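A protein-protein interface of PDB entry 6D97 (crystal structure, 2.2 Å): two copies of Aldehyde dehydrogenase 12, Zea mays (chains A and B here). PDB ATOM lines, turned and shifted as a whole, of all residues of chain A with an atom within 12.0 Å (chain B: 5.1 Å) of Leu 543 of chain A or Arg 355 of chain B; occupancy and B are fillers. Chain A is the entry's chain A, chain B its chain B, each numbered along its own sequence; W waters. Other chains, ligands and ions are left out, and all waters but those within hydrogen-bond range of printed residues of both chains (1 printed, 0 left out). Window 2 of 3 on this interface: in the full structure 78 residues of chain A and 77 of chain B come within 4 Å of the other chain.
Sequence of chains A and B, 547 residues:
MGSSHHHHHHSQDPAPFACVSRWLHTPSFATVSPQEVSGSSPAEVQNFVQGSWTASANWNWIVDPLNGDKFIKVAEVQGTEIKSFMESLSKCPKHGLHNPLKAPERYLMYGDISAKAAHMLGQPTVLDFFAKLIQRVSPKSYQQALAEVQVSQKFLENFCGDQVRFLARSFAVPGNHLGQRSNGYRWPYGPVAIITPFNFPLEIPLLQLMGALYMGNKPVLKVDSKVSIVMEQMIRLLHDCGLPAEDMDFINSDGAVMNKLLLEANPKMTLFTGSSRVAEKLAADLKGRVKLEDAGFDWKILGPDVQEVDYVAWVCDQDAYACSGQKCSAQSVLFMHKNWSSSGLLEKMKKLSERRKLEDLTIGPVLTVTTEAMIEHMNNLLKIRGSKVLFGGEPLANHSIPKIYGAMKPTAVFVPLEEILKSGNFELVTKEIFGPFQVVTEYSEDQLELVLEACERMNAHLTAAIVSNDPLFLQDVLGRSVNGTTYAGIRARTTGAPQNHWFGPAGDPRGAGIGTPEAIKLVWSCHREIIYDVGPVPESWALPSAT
No position is printed for both chains. Of the 11 pairs that touch across the chains among the printed residues, none has its exchanged pair printed and touching as well.
Among the printed residues, merely in contact across the chains: Trp 541 of chain A with Trp 314 of chain B, Leu 543 of chain A with Trp 314 of chain B, Leu 543 of chain A with Leu 352 of chain B, Leu 543 of chain A with Arg 355 of chain B, Pro 544 of chain A with Trp 314 of chain B, Ser 545 of chain A with Arg 355 of chain B, Ala 546 of chain A with Thr 362 of chain B and Thr 547 of chain A with Thr 362 of chain B.
Water W1 bridges the backbone carbonyl oxygen (O) of Ser 545 of chain A (2.5 Å) and the indole nitrogen (NE1) of Trp 314 of chain B (3.1 Å).
The guanidinium group (NH1) of Arg 356 of chain B is in salt-bridge range of the chain-end carboxylate (O) of Thr 547 of chain A (2.9 Å). The backbone NH (N) of Ala 546 of chain A sits close to the guanidinium group (NH2) of Arg 355 of chain B, at 3.4 Å. The backbone carbonyl oxygen (O) of Pro 544 of chain A lies within hydrogen-bond range of the guanidinium group (NH2) of Arg 355 of chain B (2.7 Å).
The backbone carbonyl oxygen (O) of Thr 362 of chain B lies within hydrogen-bond range of the guanidinium group (NH1) of Arg 356 of chain B (2.9 Å). N of Lys 357 of chain B is in hydrogen-bond range of OG1 of Thr 362 of chain B.
Printed residues of chain B that touch a printed residue of chain A: Trp 314, Leu 352, Arg 355, Arg 356 and Thr 362. Hydrophobic or aromatic side chains of chain B within 4 Å of the printed part of chain A: Trp 314 and Leu 352. Of the 11 printed residues of chain A, 6 touch a printed residue of chain B. Printed residues of chain A that touch a printed residue of chain B: Trp 541, Leu 543, Pro 544, Ser 545, Ala 546 and Thr 547. Among the printed residues, 11 pairs touch across the chains.
Of chain B, only Trp 314 (3.7 Å), Leu 352 (3.8 Å) and Arg 355 (3.7 Å) come within 4 Å of Leu 543 of chain A. Arg 355 of chain B touches four residues of chain A. Trp 314 of chain B touches just these residues of chain A: Trp 541, Leu 543 and Pro 544. Leu 352 of chain B touches one residue of chain A. Ser 353 of chain B touches none of the printed residues of chain A. Arg 356 of chain B touches just one residue of chain A: Thr 547 (2.9 Å). No residue of chain A comes within 4 Å of Lys 357 of chain B. Of chain A, only Ala 546 and Thr 547 come within 4 Å of Thr 362 of chain B. Of the printed residues of chain B, Trp 541 of chain A touches Trp 314 (3.7 Å). Of the printed residues of chain B, Ser 545 of chain A touches Arg 355. Of the printed residues of chain B, Ala 546 of chain A touches Arg 355 and Thr 362. Of the printed residues of chain B, Pro 544 of chain A touches Trp 314 and Arg 355. Ala 542 of chain A touches none of the printed residues of chain B. The nearest residue of chain A that does not touch Arg 355 of chain B is Thr 547 of chain A (5.8 Å). The nearest printed residue of chain B that does not touch Ser 545 of chain A is Trp 314 of chain B (5.1 Å).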
ATOM      1  N   VAL A 537      -0.925   5.439  26.809  1.00  0.00           N
ATOM      2  CA  VAL A 537      -0.692   6.850  26.521  1.00  0.00           C
ATOM      3  C   VAL A 537      -1.879   7.278  25.668  1.00  0.00           C
ATOM      4  O   VAL A 537      -2.165   6.636  24.647  1.00  0.00           O
ATOM      5  CB  VAL A 537       0.649   7.088  25.805  1.00  0.00           C
ATOM      6  CG1 VAL A 537       0.787   8.555  25.402  1.00  0.00           C
ATOM      7  CG2 VAL A 537       1.806   6.667  26.688  1.00  0.00           C
ATOM      8  N   PRO A 538      -2.612   8.315  26.061  1.00  0.00           N
ATOM      9  CA  PRO A 538      -3.807   8.703  25.306  1.00  0.00           C
ATOM     10  C   PRO A 538      -3.483   8.920  23.836  1.00  0.00           C
ATOM     11  O   PRO A 538      -2.424   9.442  23.483  1.00  0.00           O
ATOM     12  CB  PRO A 538      -4.247  10.002  25.986  1.00  0.00           C
ATOM     13  CG  PRO A 538      -3.709   9.891  27.377  1.00  0.00           C
ATOM     14  CD  PRO A 538      -2.408   9.151  27.258  1.00  0.00           C
ATOM     15  N   GLU A 539      -4.400   8.481  22.971  1.00  0.00           N
ATOM     16  CA  GLU A 539      -4.199   8.659  21.539  1.00  0.00           C
ATOM     17  C   GLU A 539      -4.062  10.131  21.183  1.00  0.00           C
ATOM     18  O   GLU A 539      -3.324  10.482  20.255  1.00  0.00           O
ATOM     19  CB  GLU A 539      -5.355   8.030  20.763  1.00  0.00           C
ATOM     20  CG  GLU A 539      -4.922   7.254  19.532  1.00  0.00           C
ATOM     21  CD  GLU A 539      -4.123   6.016  19.885  1.00  0.00           C
ATOM     22  OE1 GLU A 539      -4.633   5.184  20.667  1.00  0.00           O
ATOM     23  OE2 GLU A 539      -2.981   5.883  19.392  1.00  0.00           O
ATOM     24  N   SER A 540      -4.753  11.000  21.914  1.00  0.00           N
ATOM     25  CA  SER A 540      -4.715  12.438  21.697  1.00  0.00           C
ATOM     26  C   SER A 540      -3.525  13.109  22.368  1.00  0.00           C
ATOM     27  O   SER A 540      -3.471  14.345  22.395  1.00  0.00           O
ATOM     28  CB  SER A 540      -6.013  13.071  22.205  1.00  0.00           C
ATOM     29  OG  SER A 540      -6.256  12.711  23.555  1.00  0.00           O
ATOM     30  N   TRP A 541      -2.585  12.345  22.918  1.00  0.00           N
ATOM     31  CA  TRP A 541      -1.467  12.956  23.623  1.00  0.00           C
ATOM     32  C   TRP A 541      -0.554  13.682  22.647  1.00  0.00           C
ATOM     33  O   TRP A 541      -0.189  13.144  21.597  1.00  0.00           O
ATOM     34  CB  TRP A 541      -0.664  11.917  24.401  1.00  0.00           C
ATOM     35  CG  TRP A 541       0.439  12.554  25.204  1.00  0.00           C
ATOM     36  CD1 TRP A 541       0.320  13.139  26.432  1.00  0.00           C
ATOM     37  CD2 TRP A 541       1.817  12.691  24.826  1.00  0.00           C
ATOM     38  NE1 TRP A 541       1.538  13.621  26.847  1.00  0.00           N
ATOM     39  CE2 TRP A 541       2.473  13.360  25.880  1.00  0.00           C
ATOM     40  CE3 TRP A 541       2.562  12.311  23.702  1.00  0.00           C
ATOM     41  CZ2 TRP A 541       3.835  13.657  25.843  1.00  0.00           C
ATOM     42  CZ3 TRP A 541       3.917  12.605  23.670  1.00  0.00           C
ATOM     43  CH2 TRP A 541       4.538  13.270  24.735  1.00  0.00           C
ATOM     44  N   ALA A 542      -0.187  14.910  23.002  1.00  0.00           N
ATOM     45  CA  ALA A 542       0.757  15.708  22.238  1.00  0.00           C
ATOM     46  C   ALA A 542       1.721  16.370  23.206  1.00  0.00           C
ATOM     47  O   ALA A 542       1.312  16.851  24.266  1.00  0.00           O
ATOM     48  CB  ALA A 542       0.051  16.773  21.388  1.00  0.00           C
ATOM     49  N   LEU A 543       3.000  16.379  22.830  1.00  0.00           N
ATOM     50  CA  LEU A 543       4.083  16.952  23.618  1.00  0.00           C
ATOM     51  C   LEU A 543       3.696  18.323  24.153  1.00  0.00           C
ATOM     52  O   LEU A 543       3.557  19.275  23.374  1.00  0.00           O
ATOM     53  CB  LEU A 543       5.354  17.059  22.775  1.00  0.00           C
ATOM     54  CG  LEU A 543       6.564  17.710  23.447  1.00  0.00           C
ATOM     55  CD1 LEU A 543       7.162  16.772  24.486  1.00  0.00           C
ATOM     56  CD2 LEU A 543       7.608  18.111  22.416  1.00  0.00           C
ATOM     57  N   PRO A 544       3.498  18.464  25.460  1.00  0.00           N
ATOM     58  CA  PRO A 544       3.162  19.777  26.011  1.00  0.00           C
ATOM     59  C   PRO A 544       4.388  20.671  26.044  1.00  0.00           C
ATOM     60  O   PRO A 544       5.527  20.221  25.895  1.00  0.00           O
ATOM     61  CB  PRO A 544       2.664  19.466  27.429  1.00  0.00           C
ATOM     62  CG  PRO A 544       2.843  17.971  27.630  1.00  0.00           C
ATOM     63  CD  PRO A 544       3.698  17.459  26.516  1.00  0.00           C
ATOM     64  N   SER A 545       4.133  21.965  26.234  1.00  0.00           N
ATOM     65  CA  SER A 545       5.223  22.903  26.451  1.00  0.00           C
ATOM     66  C   SER A 545       5.958  22.546  27.735  1.00  0.00           C
ATOM     67  O   SER A 545       5.392  21.951  28.656  1.00  0.00           O
ATOM     68  CB  SER A 545       4.696  24.337  26.521  1.00  0.00           C
ATOM     69  OG  SER A 545       4.222  24.763  25.257  1.00  0.00           O
ATOM     70  N   ALA A 546       7.239  22.901  27.783  1.00  0.00           N
ATOM     71  CA  ALA A 546       8.060  22.561  28.935  1.00  0.00           C
ATOM     72  C   ALA A 546       7.550  23.263  30.190  1.00  0.00           C
ATOM     73  O   ALA A 546       6.996  24.365  30.136  1.00  0.00           O
ATOM     74  CB  ALA A 546       9.518  22.939  28.678  1.00  0.00           C
ATOM     75  N   THR A 547       7.725  22.600  31.329  1.00  0.00           N
ATOM     76  CA  THR A 547       7.483  23.223  32.626  1.00  0.00           C
ATOM     77  C   THR A 547       8.668  22.926  33.544  1.00  0.00           C
ATOM     78  O   THR A 547       9.410  21.971  33.311  1.00  0.00           O
ATOM     79  CB  THR A 547       6.181  22.723  33.291  1.00  0.00           C
ATOM     80  OG1 THR A 547       6.350  21.366  33.715  1.00  0.00           O
ATOM     81  CG2 THR A 547       5.005  22.812  32.328  1.00  0.00           C
ATOM     82  OXT THR A 547       8.915  23.612  34.537  1.00  0.00           O
ATOM     83  N   TRP B 314       9.726  12.744  26.999  1.00  0.00           N
ATOM     84  CA  TRP B 314       9.137  13.884  27.691  1.00  0.00           C
ATOM     85  C   TRP B 314       9.235  13.714  29.201  1.00  0.00           C
ATOM     86  O   TRP B 314       9.634  14.636  29.921  1.00  0.00           O
ATOM     87  CB  TRP B 314       7.682  14.058  27.254  1.00  0.00           C
ATOM     88  CG  TRP B 314       6.907  15.037  28.074  1.00  0.00           C
ATOM     89  CD1 TRP B 314       7.092  16.391  28.134  1.00  0.00           C
ATOM     90  CD2 TRP B 314       5.802  14.743  28.936  1.00  0.00           C
ATOM     91  NE1 TRP B 314       6.175  16.954  28.989  1.00  0.00           N
ATOM     92  CE2 TRP B 314       5.372  15.964  29.496  1.00  0.00           C
ATOM     93  CE3 TRP B 314       5.132  13.565  29.291  1.00  0.00           C
ATOM     94  CZ2 TRP B 314       4.307  16.040  30.392  1.00  0.00           C
ATOM     95  CZ3 TRP B 314       4.078  13.643  30.185  1.00  0.00           C
ATOM     96  CH2 TRP B 314       3.673  14.873  30.722  1.00  0.00           C
ATOM     97  N   LYS B 351      17.005  17.396  22.386  1.00  0.00           N
ATOM     98  CA  LYS B 351      16.154  18.448  21.836  1.00  0.00           C
ATOM     99  C   LYS B 351      15.266  19.054  22.913  1.00  0.00           C
ATOM    100  O   LYS B 351      15.111  20.279  22.989  1.00  0.00           O
ATOM    101  CB  LYS B 351      15.307  17.893  20.688  1.00  0.00           C
ATOM    102  CG  LYS B 351      16.065  17.780  19.379  1.00  0.00           C
ATOM    103  CD  LYS B 351      15.313  16.947  18.353  1.00  0.00           C
ATOM    104  CE  LYS B 351      16.146  16.761  17.095  1.00  0.00           C
ATOM    105  NZ  LYS B 351      15.580  15.738  16.180  1.00  0.00           N
ATOM    106  N   LEU B 352      14.680  18.208  23.763  1.00  0.00           N
ATOM    107  CA  LEU B 352      13.790  18.703  24.810  1.00  0.00           C
ATOM    108  C   LEU B 352      14.543  19.556  25.823  1.00  0.00           C
ATOM    109  O   LEU B 352      14.021  20.572  26.297  1.00  0.00           O
ATOM    110  CB  LEU B 352      13.093  17.533  25.500  1.00  0.00           C
ATOM    111  CG  LEU B 352      12.053  16.782  24.670  1.00  0.00           C
ATOM    112  CD1 LEU B 352      11.682  15.483  25.355  1.00  0.00           C
ATOM    113  CD2 LEU B 352      10.825  17.641  24.468  1.00  0.00           C
ATOM    114  N   SER B 353      15.773  19.162  26.170  1.00  0.00           N
ATOM    115  CA  SER B 353      16.561  19.957  27.107  1.00  0.00           C
ATOM    116  C   SER B 353      16.875  21.339  26.545  1.00  0.00           C
ATOM    117  O   SER B 353      16.939  22.316  27.299  1.00  0.00           O
ATOM    118  CB  SER B 353      17.858  19.227  27.461  1.00  0.00           C
ATOM    119  OG  SER B 353      18.819  19.358  26.428  1.00  0.00           O
ATOM    120  N   GLU B 354      17.054  21.444  25.228  1.00  0.00           N
ATOM    121  CA  GLU B 354      17.498  22.688  24.613  1.00  0.00           C
ATOM    122  C   GLU B 354      16.376  23.696  24.399  1.00  0.00           C
ATOM    123  O   GLU B 354      16.666  24.847  24.053  1.00  0.00           O
ATOM    124  CB  GLU B 354      18.197  22.385  23.285  1.00  0.00           C
ATOM    125  CG  GLU B 354      19.548  21.719  23.473  1.00  0.00           C
ATOM    126  CD  GLU B 354      20.072  21.065  22.208  1.00  0.00           C
ATOM    127  OE1 GLU B 354      21.270  20.711  22.180  1.00  0.00           O
ATOM    128  OE2 GLU B 354      19.288  20.900  21.249  1.00  0.00           O
ATOM    129  N   ARG B 355      15.115  23.311  24.592  1.00  0.00           N
ATOM    130  CA  ARG B 355      14.031  24.285  24.577  1.00  0.00           C
ATOM    131  C   ARG B 355      13.749  24.858  25.958  1.00  0.00           C
ATOM    132  O   ARG B 355      12.883  25.731  26.086  1.00  0.00           O
ATOM    133  CB  ARG B 355      12.749  23.674  23.991  1.00  0.00           C
ATOM    134  CG  ARG B 355      12.075  22.664  24.883  1.00  0.00           C
ATOM    135  CD  ARG B 355      10.712  22.242  24.340  1.00  0.00           C
ATOM    136  NE  ARG B 355      10.027  21.350  25.274  1.00  0.00           N
ATOM    137  CZ  ARG B 355       8.765  20.948  25.149  1.00  0.00           C
ATOM    138  NH1 ARG B 355       8.031  21.350  24.121  1.00  0.00           N
ATOM    139  NH2 ARG B 355       8.236  20.140  26.058  1.00  0.00           N
ATOM    140  N   ARG B 356      14.459  24.399  26.985  1.00  0.00           N
ATOM    141  CA  ARG B 356      14.348  25.011  28.302  1.00  0.00           C
ATOM    142  C   ARG B 356      15.088  26.341  28.314  1.00  0.00           C
ATOM    143  O   ARG B 356      16.196  26.458  27.783  1.00  0.00           O
ATOM    144  CB  ARG B 356      14.898  24.071  29.374  1.00  0.00           C
ATOM    145  CG  ARG B 356      14.168  22.742  29.394  1.00  0.00           C
ATOM    146  CD  ARG B 356      14.432  21.913  30.640  1.00  0.00           C
ATOM    147  NE  ARG B 356      13.390  20.900  30.792  1.00  0.00           N
ATOM    148  CZ  ARG B 356      12.305  21.046  31.546  1.00  0.00           C
ATOM    149  NH1 ARG B 356      12.123  22.163  32.241  1.00  0.00           N
ATOM    150  NH2 ARG B 356      11.406  20.070  31.608  1.00  0.00           N
ATOM    151  N   LYS B 357      14.460  27.353  28.908  1.00  0.00           N
ATOM    152  CA  LYS B 357      14.969  28.712  28.822  1.00  0.00           C
ATOM    153  C   LYS B 357      14.659  29.454  30.113  1.00  0.00           C
ATOM    154  O   LYS B 357      13.740  29.091  30.854  1.00  0.00           O
ATOM    155  CB  LYS B 357      14.371  29.451  27.620  1.00  0.00           C
ATOM    156  CG  LYS B 357      12.866  29.279  27.479  1.00  0.00           C
ATOM    157  CD  LYS B 357      12.359  30.013  26.257  1.00  0.00           C
ATOM    158  CE  LYS B 357      10.874  29.796  26.047  1.00  0.00           C
ATOM    159  NZ  LYS B 357      10.560  28.401  25.634  1.00  0.00           N
ATOM    160  N   THR B 362      11.906  27.410  32.826  1.00  0.00           N
ATOM    161  CA  THR B 362      12.103  25.993  32.566  1.00  0.00           C
ATOM    162  C   THR B 362      13.559  25.579  32.729  1.00  0.00           C
ATOM    163  O   THR B 362      13.858  24.380  32.735  1.00  0.00           O
ATOM    164  CB  THR B 362      11.596  25.639  31.167  1.00  0.00           C
ATOM    165  OG1 THR B 362      12.063  26.611  30.222  1.00  0.00           O
ATOM    166  CG2 THR B 362      10.079  25.614  31.159  1.00  0.00           C
HETATM  167  O   HOH W   1       5.720  19.857  30.020  1.00  0.00           O
